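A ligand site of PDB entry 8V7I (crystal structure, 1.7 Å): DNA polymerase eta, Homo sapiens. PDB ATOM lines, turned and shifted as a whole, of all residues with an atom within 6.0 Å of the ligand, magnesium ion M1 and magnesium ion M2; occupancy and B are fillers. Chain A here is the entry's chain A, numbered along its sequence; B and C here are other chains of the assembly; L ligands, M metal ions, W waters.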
ATOM      1  N   ASP A  16     -18.956  17.283  36.484  1.00  0.00           N
ATOM      2  CA  ASP A  16     -18.418  16.789  35.221  1.00  0.00           C
ATOM      3  C   ASP A  16     -19.599  16.692  34.256  1.00  0.00           C
ATOM      4  O   ASP A  16     -20.590  16.005  34.552  1.00  0.00           O
ATOM      5  CB  ASP A  16     -17.754  15.430  35.435  1.00  0.00           C
ATOM      6  CG  ASP A  16     -17.263  14.798  34.168  1.00  0.00           C
ATOM      7  OD1 ASP A  16     -18.023  14.706  33.188  1.00  0.00           O
ATOM      8  OD2 ASP A  16     -16.089  14.381  34.183  1.00  0.00           O
ATOM      9  N   MET A  17     -19.499  17.346  33.115  1.00  0.00           N
ATOM     10  CA  MET A  17     -20.551  17.174  32.126  1.00  0.00           C
ATOM     11  C   MET A  17     -20.476  15.804  31.476  1.00  0.00           C
ATOM     12  O   MET A  17     -19.431  15.417  30.946  1.00  0.00           O
ATOM     13  CB  MET A  17     -20.511  18.282  31.076  1.00  0.00           C
ATOM     14  CG  MET A  17     -19.961  19.570  31.598  1.00  0.00           C
ATOM     15  SD  MET A  17     -21.354  20.174  32.633  1.00  0.00           S
ATOM     16  CE  MET A  17     -22.704  20.236  31.468  1.00  0.00           C
ATOM     17  N   ASP A  18     -21.597  15.083  31.525  1.00  0.00           N
ATOM     18  CA  ASP A  18     -21.717  13.772  30.884  1.00  0.00           C
ATOM     19  C   ASP A  18     -21.424  13.879  29.397  1.00  0.00           C
ATOM     20  O   ASP A  18     -21.972  14.760  28.729  1.00  0.00           O
ATOM     21  CB  ASP A  18     -23.147  13.245  31.088  1.00  0.00           C
ATOM     22  CG  ASP A  18     -23.509  13.068  32.560  1.00  0.00           C
ATOM     23  OD1 ASP A  18     -22.615  12.849  33.376  1.00  0.00           O
ATOM     24  OD2 ASP A  18     -24.700  13.151  32.892  1.00  0.00           O
ATOM     25  N   CYS A  19     -20.569  12.984  28.887  1.00  0.00           N
ATOM     26  CA  CYS A  19     -20.166  12.911  27.474  1.00  0.00           C
ATOM     27  C   CYS A  19     -20.333  14.246  26.765  1.00  0.00           C
ATOM     28  O   CYS A  19     -21.158  14.385  25.857  1.00  0.00           O
ATOM     29  CB  CYS A  19     -20.948  11.809  26.757  1.00  0.00           C
ATOM     30  SG  CYS A  19     -22.722  11.803  27.039  1.00  0.00           S
ATOM     31  N   PHE A  20     -19.518  15.225  27.158  1.00  0.00           N
ATOM     32  CA  PHE A  20     -19.842  16.627  26.903  1.00  0.00           C
ATOM     33  C   PHE A  20     -19.970  16.943  25.411  1.00  0.00           C
ATOM     34  O   PHE A  20     -20.957  17.560  24.981  1.00  0.00           O
ATOM     35  CB  PHE A  20     -18.793  17.520  27.543  1.00  0.00           C
ATOM     36  CG  PHE A  20     -19.108  18.972  27.416  1.00  0.00           C
ATOM     37  CD1 PHE A  20     -20.384  19.437  27.687  1.00  0.00           C
ATOM     38  CD2 PHE A  20     -18.133  19.867  26.964  1.00  0.00           C
ATOM     39  CE1 PHE A  20     -20.690  20.799  27.538  1.00  0.00           C
ATOM     40  CE2 PHE A  20     -18.428  21.214  26.830  1.00  0.00           C
ATOM     41  CZ  PHE A  20     -19.692  21.672  27.118  1.00  0.00           C
ATOM     42  N   PHE A  21     -18.955  16.587  24.608  1.00  0.00           N
ATOM     43  CA  PHE A  21     -19.019  16.937  23.191  1.00  0.00           C
ATOM     44  C   PHE A  21     -20.256  16.336  22.534  1.00  0.00           C
ATOM     45  O   PHE A  21     -20.880  16.965  21.669  1.00  0.00           O
ATOM     46  CB  PHE A  21     -17.772  16.462  22.433  1.00  0.00           C
ATOM     47  CG  PHE A  21     -16.510  17.227  22.752  1.00  0.00           C
ATOM     48  CD1 PHE A  21     -16.415  18.047  23.881  1.00  0.00           C
ATOM     49  CD2 PHE A  21     -15.421  17.134  21.895  1.00  0.00           C
ATOM     50  CE1 PHE A  21     -15.227  18.742  24.149  1.00  0.00           C
ATOM     51  CE2 PHE A  21     -14.236  17.837  22.174  1.00  0.00           C
ATOM     52  CZ  PHE A  21     -14.151  18.622  23.280  1.00  0.00           C
ATOM     53  N   VAL A  22     -20.612  15.101  22.937  1.00  0.00           N
ATOM     54  CA  VAL A  22     -21.842  14.474  22.464  1.00  0.00           C
ATOM     55  C   VAL A  22     -23.061  15.295  22.860  1.00  0.00           C
ATOM     56  O   VAL A  22     -23.969  15.515  22.049  1.00  0.00           O
ATOM     57  CB  VAL A  22     -21.958  13.038  22.994  1.00  0.00           C
ATOM     58  CG1 VAL A  22     -23.347  12.482  22.746  1.00  0.00           C
ATOM     59  CG2 VAL A  22     -20.943  12.140  22.316  1.00  0.00           C
ATOM     60  N   GLN A  41     -13.191  12.862  15.301  1.00  0.00           N
ATOM     61  CA  GLN A  41     -12.299  13.886  14.712  1.00  0.00           C
ATOM     62  C   GLN A  41     -11.717  13.260  13.450  1.00  0.00           C
ATOM     63  O   GLN A  41     -11.200  12.142  13.535  1.00  0.00           O
ATOM     64  CB  GLN A  41     -11.167  14.266  15.653  1.00  0.00           C
ATOM     65  CG  GLN A  41     -11.455  15.422  16.578  1.00  0.00           C
ATOM     66  CD  GLN A  41     -10.340  15.658  17.565  1.00  0.00           C
ATOM     67  OE1 GLN A  41     -10.262  16.707  18.197  1.00  0.00           O
ATOM     68  NE2 GLN A  41      -9.473  14.672  17.710  1.00  0.00           N
ATOM     69  N   ILE A  51     -13.845  10.557  19.990  1.00  0.00           N
ATOM     70  CA  ILE A  51     -13.395  11.301  21.168  1.00  0.00           C
ATOM     71  C   ILE A  51     -14.487  11.482  22.222  1.00  0.00           C
ATOM     72  O   ILE A  51     -14.159  11.883  23.346  1.00  0.00           O
ATOM     73  CB  ILE A  51     -12.787  12.656  20.759  1.00  0.00           C
ATOM     74  CG1 ILE A  51     -13.801  13.509  20.022  1.00  0.00           C
ATOM     75  CG2 ILE A  51     -11.543  12.447  19.896  1.00  0.00           C
ATOM     76  CD1 ILE A  51     -13.309  14.869  19.782  1.00  0.00           C
ATOM     77  N   ALA A  52     -15.744  11.158  21.923  1.00  0.00           N
ATOM     78  CA  ALA A  52     -16.776  11.193  22.984  1.00  0.00           C
ATOM     79  C   ALA A  52     -17.925  10.242  22.635  1.00  0.00           C
ATOM     80  O   ALA A  52     -18.244  10.057  21.472  1.00  0.00           O
ATOM     81  CB  ALA A  52     -17.336  12.612  23.179  1.00  0.00           C
ATOM     82  N   VAL A  53     -18.539   9.641  23.661  1.00  0.00           N
ATOM     83  CA  VAL A  53     -19.478   8.539  23.457  1.00  0.00           C
ATOM     84  C   VAL A  53     -20.689   8.691  24.362  1.00  0.00           C
ATOM     85  O   VAL A  53     -20.543   8.795  25.579  1.00  0.00           O
ATOM     86  CB  VAL A  53     -18.799   7.183  23.736  1.00  0.00           C
ATOM     87  CG1 VAL A  53     -19.707   6.064  23.292  1.00  0.00           C
ATOM     88  CG2 VAL A  53     -17.504   7.102  23.002  1.00  0.00           C
ATOM     89  N   TYR A  55     -24.060   7.509  26.435  1.00  0.00           N
ATOM     90  CA  TYR A  55     -24.136   6.326  27.304  1.00  0.00           C
ATOM     91  C   TYR A  55     -24.839   5.176  26.610  1.00  0.00           C
ATOM     92  O   TYR A  55     -24.486   4.005  26.839  1.00  0.00           O
ATOM     93  CB  TYR A  55     -24.795   6.697  28.632  1.00  0.00           C
ATOM     94  CG  TYR A  55     -23.792   7.376  29.578  1.00  0.00           C
ATOM     95  CD1 TYR A  55     -23.394   8.701  29.372  1.00  0.00           C
ATOM     96  CD2 TYR A  55     -23.183   6.670  30.594  1.00  0.00           C
ATOM     97  CE1 TYR A  55     -22.482   9.325  30.215  1.00  0.00           C
ATOM     98  CE2 TYR A  55     -22.242   7.269  31.436  1.00  0.00           C
ATOM     99  CZ  TYR A  55     -21.891   8.585  31.251  1.00  0.00           C
ATOM    100  OH  TYR A  55     -20.959   9.149  32.116  1.00  0.00           O
ATOM    101  N   ARG A  58     -22.011   3.589  24.740  1.00  0.00           N
ATOM    102  CA  ARG A  58     -21.121   2.864  25.662  1.00  0.00           C
ATOM    103  C   ARG A  58     -21.665   1.487  25.998  1.00  0.00           C
ATOM    104  O   ARG A  58     -20.873   0.545  26.179  1.00  0.00           O
ATOM    105  CB  ARG A  58     -20.902   3.659  26.944  1.00  0.00           C
ATOM    106  CG  ARG A  58     -20.190   4.967  26.743  1.00  0.00           C
ATOM    107  CD  ARG A  58     -20.038   5.706  28.037  1.00  0.00           C
ATOM    108  NE  ARG A  58     -19.715   7.108  27.816  1.00  0.00           N
ATOM    109  CZ  ARG A  58     -19.244   7.919  28.754  1.00  0.00           C
ATOM    110  NH1 ARG A  58     -19.022   7.486  29.989  1.00  0.00           N
ATOM    111  NH2 ARG A  58     -18.986   9.194  28.455  1.00  0.00           N
ATOM    112  N   ARG A  64     -13.877   5.894  23.910  1.00  0.00           N
ATOM    113  CA  ARG A  64     -13.011   6.929  23.333  1.00  0.00           C
ATOM    114  C   ARG A  64     -11.760   6.241  22.804  1.00  0.00           C
ATOM    115  O   ARG A  64     -11.455   5.130  23.281  1.00  0.00           O
ATOM    116  CB  ARG A  64     -12.586   7.910  24.412  1.00  0.00           C
ATOM    117  CG  ARG A  64     -12.439   9.362  23.969  1.00  0.00           C
ATOM    118  CD  ARG A  64     -12.287  10.255  25.186  1.00  0.00           C
ATOM    119  NE  ARG A  64     -11.753   9.494  26.302  1.00  0.00           N
ATOM    120  CZ  ARG A  64     -12.298   9.450  27.517  1.00  0.00           C
ATOM    121  NH1 ARG A  64     -13.394  10.131  27.772  1.00  0.00           N
ATOM    122  NH2 ARG A  64     -11.741   8.726  28.468  1.00  0.00           N
ATOM    123  N   SER A 116     -10.917  21.219  33.500  1.00  0.00           N
ATOM    124  CA  SER A 116     -10.791  20.917  32.084  1.00  0.00           C
ATOM    125  C   SER A 116     -12.012  21.490  31.384  1.00  0.00           C
ATOM    126  O   SER A 116     -12.909  22.021  32.040  1.00  0.00           O
ATOM    127  CB  SER A 116     -10.659  19.410  31.830  1.00  0.00           C
ATOM    128  OG  SER A 116     -11.923  18.788  31.900  1.00  0.00           O
ATOM    129  N   ILE A 117     -12.065  21.317  30.056  1.00  0.00           N
ATOM    130  CA  ILE A 117     -13.180  21.851  29.279  1.00  0.00           C
ATOM    131  C   ILE A 117     -14.527  21.431  29.843  1.00  0.00           C
ATOM    132  O   ILE A 117     -15.519  22.146  29.690  1.00  0.00           O
ATOM    133  CB  ILE A 117     -13.070  21.444  27.792  1.00  0.00           C
ATOM    134  CG1 ILE A 117     -14.006  22.312  26.949  1.00  0.00           C
ATOM    135  CG2 ILE A 117     -13.462  20.001  27.590  1.00  0.00           C
ATOM    136  CD1 ILE A 117     -13.635  22.333  25.467  1.00  0.00           C
ATOM    137  N   ASP A 118     -14.604  20.263  30.486  1.00  0.00           N
ATOM    138  CA  ASP A 118     -15.907  19.779  30.902  1.00  0.00           C
ATOM    139  C   ASP A 118     -15.940  19.447  32.386  1.00  0.00           C
ATOM    140  O   ASP A 118     -16.813  18.687  32.823  1.00  0.00           O
ATOM    141  CB  ASP A 118     -16.315  18.555  30.123  1.00  0.00           C
ATOM    142  CG  ASP A 118     -15.724  17.316  30.696  1.00  0.00           C
ATOM    143  OD1 ASP A 118     -14.493  17.276  30.965  1.00  0.00           O
ATOM    144  OD2 ASP A 118     -16.544  16.408  30.942  1.00  0.00           O
ATOM    145  N   GLU A 119     -15.030  19.988  33.190  1.00  0.00           N
ATOM    146  CA  GLU A 119     -15.022  19.594  34.604  1.00  0.00           C
ATOM    147  C   GLU A 119     -14.616  20.808  35.427  1.00  0.00           C
ATOM    148  O   GLU A 119     -13.688  21.471  35.013  1.00  0.00           O
ATOM    149  CB  GLU A 119     -13.948  18.544  34.802  1.00  0.00           C
ATOM    150  CG  GLU A 119     -14.377  17.416  35.699  1.00  0.00           C
ATOM    151  CD  GLU A 119     -13.339  16.320  35.641  1.00  0.00           C
ATOM    152  OE1 GLU A 119     -12.244  16.538  36.168  1.00  0.00           O
ATOM    153  OE2 GLU A 119     -13.613  15.280  35.044  1.00  0.00           O
ATOM    154  N   LYS A 227     -13.943  14.046  43.235  1.00  0.00           N
ATOM    155  CA  LYS A 227     -13.798  13.492  41.902  1.00  0.00           C
ATOM    156  C   LYS A 227     -14.076  11.983  41.899  1.00  0.00           C
ATOM    157  O   LYS A 227     -14.781  11.454  41.011  1.00  0.00           O
ATOM    158  CB  LYS A 227     -12.401  13.818  41.394  1.00  0.00           C
ATOM    159  CG  LYS A 227     -11.927  12.997  40.224  1.00  0.00           C
ATOM    160  CD  LYS A 227     -12.539  13.514  38.968  1.00  0.00           C
ATOM    161  CE  LYS A 227     -11.662  13.171  37.772  1.00  0.00           C
ATOM    162  NZ  LYS A 227     -12.328  13.534  36.495  1.00  0.00           N
ATOM    163  N   LYS A 234     -22.969   7.606  37.474  1.00  0.00           N
ATOM    164  CA  LYS A 234     -23.148   8.394  36.253  1.00  0.00           C
ATOM    165  C   LYS A 234     -24.081   7.571  35.342  1.00  0.00           C
ATOM    166  O   LYS A 234     -24.135   6.347  35.484  1.00  0.00           O
ATOM    167  CB  LYS A 234     -21.784   8.626  35.597  1.00  0.00           C
ATOM    168  CG  LYS A 234     -20.907   9.738  36.171  1.00  0.00           C
ATOM    169  CD  LYS A 234     -19.961  10.324  35.136  1.00  0.00           C
ATOM    170  CE  LYS A 234     -19.707  11.818  35.296  1.00  0.00           C
ATOM    171  NZ  LYS A 234     -19.943  12.591  34.042  1.00  0.00           N
ATOM    172  N   PRO A 235     -24.796   8.255  34.437  1.00  0.00           N
ATOM    173  CA  PRO A 235     -24.857   9.696  34.203  1.00  0.00           C
ATOM    174  C   PRO A 235     -25.964  10.384  34.980  1.00  0.00           C
ATOM    175  O   PRO A 235     -26.843   9.735  35.559  1.00  0.00           O
ATOM    176  CB  PRO A 235     -25.159   9.779  32.706  1.00  0.00           C
ATOM    177  CG  PRO A 235     -26.079   8.595  32.486  1.00  0.00           C
ATOM    178  CD  PRO A 235     -25.570   7.515  33.431  1.00  0.00           C
ATOM    179  P   CAR B   8      -9.485  12.958  34.988  1.00  0.00           P
ATOM    180  OP1 CAR B   8      -8.955  13.083  36.390  1.00  0.00           O
ATOM    181  OP2 CAR B   8     -10.797  12.205  34.942  1.00  0.00           O
ATOM    182  O5' CAR B   8      -9.616  14.425  34.229  1.00  0.00           O
ATOM    183  C5' CAR B   8     -10.887  14.879  33.825  1.00  0.00           C
ATOM    184  C4' CAR B   8     -10.910  15.606  32.459  1.00  0.00           C
ATOM    185  O4' CAR B   8      -9.750  15.048  31.836  1.00  0.00           O
ATOM    186  C3' CAR B   8     -12.062  15.145  31.563  1.00  0.00           C
ATOM    187  O3' CAR B   8     -12.470  16.248  30.800  1.00  0.00           O
ATOM    188  C2' CAR B   8     -11.421  14.180  30.583  1.00  0.00           C
ATOM    189  O2' CAR B   8     -11.240  12.889  31.147  1.00  0.00           O
ATOM    190  C1' CAR B   8     -10.079  14.908  30.458  1.00  0.00           C
ATOM    191  N1  CAR B   8      -8.998  14.253  29.730  1.00  0.00           N
ATOM    192  C2  CAR B   8      -8.479  14.858  28.574  1.00  0.00           C
ATOM    193  O2  CAR B   8      -8.949  15.922  28.173  1.00  0.00           O
ATOM    194  N3  CAR B   8      -7.463  14.287  27.884  1.00  0.00           N
ATOM    195  C4  CAR B   8      -6.929  13.138  28.293  1.00  0.00           C
ATOM    196  N4  CAR B   8      -5.938  12.601  27.606  1.00  0.00           N
ATOM    197  C5  CAR B   8      -7.428  12.505  29.466  1.00  0.00           C
ATOM    198  C6  CAR B   8      -8.437  13.065  30.158  1.00  0.00           C
ATOM    199  P    DT C   4      -2.880   9.865  16.927  1.00  0.00           P
ATOM    200  OP1  DT C   4      -2.524   9.867  15.490  1.00  0.00           O
ATOM    201  OP2  DT C   4      -1.710  10.010  17.871  1.00  0.00           O
ATOM    202  O5'  DT C   4      -3.864  11.096  17.208  1.00  0.00           O
ATOM    203  C5'  DT C   4      -5.083  11.286  16.456  1.00  0.00           C
ATOM    204  C4'  DT C   4      -5.730  12.592  16.860  1.00  0.00           C
ATOM    205  O4'  DT C   4      -6.390  12.464  18.148  1.00  0.00           O
ATOM    206  C3'  DT C   4      -4.797  13.781  17.008  1.00  0.00           C
ATOM    207  O3'  DT C   4      -5.530  14.926  16.607  1.00  0.00           O
ATOM    208  C2'  DT C   4      -4.589  13.890  18.500  1.00  0.00           C
ATOM    209  C1'  DT C   4      -5.961  13.521  19.002  1.00  0.00           C
ATOM    210  N1   DT C   4      -5.928  12.964  20.345  1.00  0.00           N
ATOM    211  C2   DT C   4      -6.933  13.289  21.229  1.00  0.00           C
ATOM    212  O2   DT C   4      -7.864  14.029  20.940  1.00  0.00           O
ATOM    213  N3   DT C   4      -6.813  12.684  22.461  1.00  0.00           N
ATOM    214  C4   DT C   4      -5.812  11.831  22.871  1.00  0.00           C
ATOM    215  O4   DT C   4      -5.842  11.378  24.003  1.00  0.00           O
ATOM    216  C5   DT C   4      -4.798  11.539  21.894  1.00  0.00           C
ATOM    217  C7   DT C   4      -3.680  10.616  22.263  1.00  0.00           C
ATOM    218  C6   DT C   4      -4.904  12.114  20.688  1.00  0.00           C
ATOM    219  P    DG C   5      -4.797  16.318  16.431  1.00  0.00           P
ATOM    220  OP1  DG C   5      -5.213  16.853  15.110  1.00  0.00           O
ATOM    221  OP2  DG C   5      -3.342  16.173  16.699  1.00  0.00           O
ATOM    222  O5'  DG C   5      -5.390  17.194  17.616  1.00  0.00           O
ATOM    223  C5'  DG C   5      -6.762  17.513  17.651  1.00  0.00           C
ATOM    224  C4'  DG C   5      -7.046  18.234  18.940  1.00  0.00           C
ATOM    225  O4'  DG C   5      -6.849  17.324  20.057  1.00  0.00           O
ATOM    226  C3'  DG C   5      -6.114  19.407  19.198  1.00  0.00           C
ATOM    227  O3'  DG C   5      -6.857  20.446  19.771  1.00  0.00           O
ATOM    228  C2'  DG C   5      -5.105  18.843  20.200  1.00  0.00           C
ATOM    229  C1'  DG C   5      -6.014  17.934  21.005  1.00  0.00           C
ATOM    230  N9   DG C   5      -5.318  16.914  21.763  1.00  0.00           N
ATOM    231  C8   DG C   5      -4.117  16.332  21.466  1.00  0.00           C
ATOM    232  N7   DG C   5      -3.737  15.459  22.368  1.00  0.00           N
ATOM    233  C5   DG C   5      -4.763  15.480  23.314  1.00  0.00           C
ATOM    234  C6   DG C   5      -4.911  14.747  24.509  1.00  0.00           C
ATOM    235  O6   DG C   5      -4.147  13.902  24.988  1.00  0.00           O
ATOM    236  N1   DG C   5      -6.093  15.080  25.173  1.00  0.00           N
ATOM    237  C2   DG C   5      -7.013  16.003  24.727  1.00  0.00           C
ATOM    238  N2   DG C   5      -8.089  16.190  25.492  1.00  0.00           N
ATOM    239  N3   DG C   5      -6.881  16.687  23.608  1.00  0.00           N
ATOM    240  C4   DG C   5      -5.730  16.378  22.953  1.00  0.00           C
HETATM  241  P1  LIG L   1     -18.320  11.330  30.900  1.00  0.00           P
HETATM  242  O1  LIG L   1     -17.728   9.996  31.229  1.00  0.00           O
HETATM  243  O2  LIG L   1     -17.675  12.449  31.673  1.00  0.00           O
HETATM  244  O3  LIG L   1     -19.813  11.341  30.990  1.00  0.00           O
HETATM  245  P2  LIG L   1     -17.164  12.827  28.711  1.00  0.00           P
HETATM  246  O4  LIG L   1     -17.589  14.125  29.313  1.00  0.00           O
HETATM  247  O5  LIG L   1     -17.129  12.683  27.217  1.00  0.00           O
HETATM  248  O6  LIG L   1     -17.977  11.628  29.370  1.00  0.00           O
HETATM  249  P3  LIG L   1     -14.613  13.337  30.004  1.00  0.00           P
HETATM  250  O7  LIG L   1     -15.249  14.106  31.102  1.00  0.00           O
HETATM  251  O8  LIG L   1     -13.513  12.392  30.348  1.00  0.00           O
HETATM  252  O9  LIG L   1     -15.710  12.466  29.262  1.00  0.00           O
HETATM  253  O10 LIG L   1     -14.151  14.341  28.828  1.00  0.00           O
HETATM  254  C1  LIG L   1     -15.015  15.475  28.550  1.00  0.00           C
HETATM  255  C2  LIG L   1     -14.927  15.914  27.103  1.00  0.00           C
HETATM  256  O11 LIG L   1     -13.552  16.224  26.798  1.00  0.00           O
HETATM  257  C3  LIG L   1     -15.394  14.883  26.084  1.00  0.00           C
HETATM  258  O12 LIG L   1     -16.730  15.143  25.705  1.00  0.00           O
HETATM  259  C4  LIG L   1     -14.454  15.100  24.903  1.00  0.00           C
HETATM  260  C5  LIG L   1     -13.196  15.652  25.539  1.00  0.00           C
HETATM  261  N1  LIG L   1     -12.181  14.658  25.795  1.00  0.00           N
HETATM  262  C6  LIG L   1     -12.000  13.887  26.905  1.00  0.00           C
HETATM  263  N2  LIG L   1     -10.954  13.100  26.812  1.00  0.00           N
HETATM  264  C7  LIG L   1     -10.420  13.383  25.564  1.00  0.00           C
HETATM  265  C8  LIG L   1      -9.320  12.885  24.861  1.00  0.00           C
HETATM  266  N3  LIG L   1      -8.478  11.959  25.323  1.00  0.00           N
HETATM  267  N4  LIG L   1      -9.087  13.406  23.631  1.00  0.00           N
HETATM  268  C9  LIG L   1      -9.906  14.334  23.147  1.00  0.00           C
HETATM  269  N5  LIG L   1     -10.975  14.872  23.713  1.00  0.00           N
HETATM  270  C10 LIG L   1     -11.168  14.348  24.929  1.00  0.00           C
HETATM  271 MG    MG M   1     -17.438  14.456  31.327  1.00  0.00          MG
HETATM  272 MG    MG M   2     -14.429  15.637  32.541  1.00  0.00          MG
HETATM  273  O   HOH W   1     -14.086  13.504  33.507  1.00  0.00           O
HETATM  274  O   HOH W   2     -17.307  10.279  26.187  1.00  0.00           O
HETATM  275  O   HOH W   3     -15.831   8.570  30.185  1.00  0.00           O
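O8 of the ligand is in salt-bridge range of NH1 of Arg 64. An oxygen (O3) of the ligand lies within salt-bridge range of the side-chain amino group (NZ) of Lys 234. A nitrogen (N3) of the ligand sits at hydrogen-bond distance from N4 of CAR 8 of chain B (3.5 Å). An oxygen (O3) of the ligand lies within hydrogen-bond range of the backbone NH (N) of Cys 19, 2.8 Å away. An oxygen (O8) of the ligand sits close to O2' of CAR 8 of chain B (2.5 Å). N3 of the ligand lies within hydrogen-bond range of O4 of DT 4 of chain C. OH of Tyr 55 lies within hydrogen-bond range of O3 of the ligand (2.7 Å). O12 of the ligand lies within hydrogen-bond range of N of Phe 20 (3.1 Å). N of Phe 21 lies within hydrogen-bond range of O12 of the ligand (2.9 Å). An oxygen (O1) of the ligand lies within salt-bridge range of the guanidinium group of Arg 58 (3.1 Å).
The side-chain amino group of Lys 234 lies within salt-bridge range of the side-chain carboxylate of Asp 18 (2.8 Å). O3' of CAR 8 of chain B lies within hydrogen-bond range of the side-chain hydroxyl (OG) of Ser 116 (2.8 Å). The backbone carbonyl oxygen (O) of Val 53 is in hydrogen-bond range of the guanidinium group (NE) of Arg 58, 2.9 Å away. The backbone NH (N) of Asp 118 lies close to the side-chain hydroxyl (OG) of Ser 116. The side-chain carboxylate (OE2) of Glu 119 is in salt-bridge range of the side-chain amino group (NZ) of Lys 227. The side-chain carboxylate (OD1) of Asp 16 lies close to the side-chain amino group (NZ) of Lys 234, 3.0 Å away. OH of Tyr 55 sits close to NH1 of Arg 58 (3.3 Å). OP2 of CAR 8 of chain B is in salt-bridge range of the side-chain amino group (NZ) of Lys 227 (2.6 Å).
N4 of the ligand lies close to N2 of DG 5 of chain C, at 3.5 Å. CA of Asp 18 touches O3 of the ligand, at 3.1 Å. O of Ile 51 touches C4 of the ligand, at 3.6 Å. CB of Ala 52 touches O12 of the ligand, at 3.6 Å. CG2 of Ile 117 touches O11 of the ligand, at 3.9 Å. Hydrophobic or aromatic side chains within 4 Å of the ligand: Phe 20, Phe 21, Ala 52, Tyr 55 and Ile 117. Within 4 Å of the ligand: Asp 16, Met 17, Asp 18, Cys 19, Phe 20, Phe 21, Ile 51, Ala 52, Tyr 55, Arg 58, Arg 64, Ile 117, Asp 118, Lys 234, CAR 8 of chain B, DT 4 of chain C and DG 5 of chain C.
Within 4 Å of magnesium ion M1: Asp 16, Met 17 and Asp 118.
Four residues have an atom within 4 Å of magnesium ion M2: Asp 16, Asp 118, Glu 119 and CAR 8 of chain B. The nearest printed residue that does not touch magnesium ion M2 is Ser 116 (4.1 Å).
OD1 of Asp 16 is bound to magnesium ion M1 (2.0 Å). O4 of the ligand is bound to magnesium ion M1 (2.0 Å). O2 of the ligand is bound to magnesium ion M1. Magnesium ion M1 is bound by the side-chain carboxylate (OD2) of Asp 118, at 2.2 Å. Magnesium ion M1 is bound by O7 of the ligand (2.2 Å). The backbone carbonyl oxygen (O) of Met 17 is bound to magnesium ion M1 (2.2 Å). Magnesium ion M1 has six donor atoms within binding distance.
Magnesium ion M2 is bound by O7 of the ligand (2.3 Å), OD1 of Asp 118 (2.3 Å) and water W1 (2.4 Å). Magnesium ion M2 has three donor atoms within binding distance. Slightly farther from magnesium ion M2 lies OD2 of Asp 16 (2.7 Å). Slightly farther from magnesium ion M2 lies OE2 of Glu 119 (2.7 Å). Slightly farther from magnesium ion M2 lies O3' of CAR 8 of chain B (2.7 Å). Slightly farther from magnesium ion M2 lies the side-chain carboxylate (OD2) of Asp 118 (2.8 Å).
Water W1 bridges an oxygen (O8) of the ligand and the side-chain amino group (NZ) of Lys 227. Water W3 lies within hydrogen-bond range of O1 of the ligand (2.6 Å) and NH1 of Arg 58 (3.4 Å). Water W2 lies within hydrogen-bond range of an oxygen (O5) of the ligand (2.6 Å), the backbone NH of Val 53 (2.9 Å) and the guanidinium group of Arg 58 (3.0 Å).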
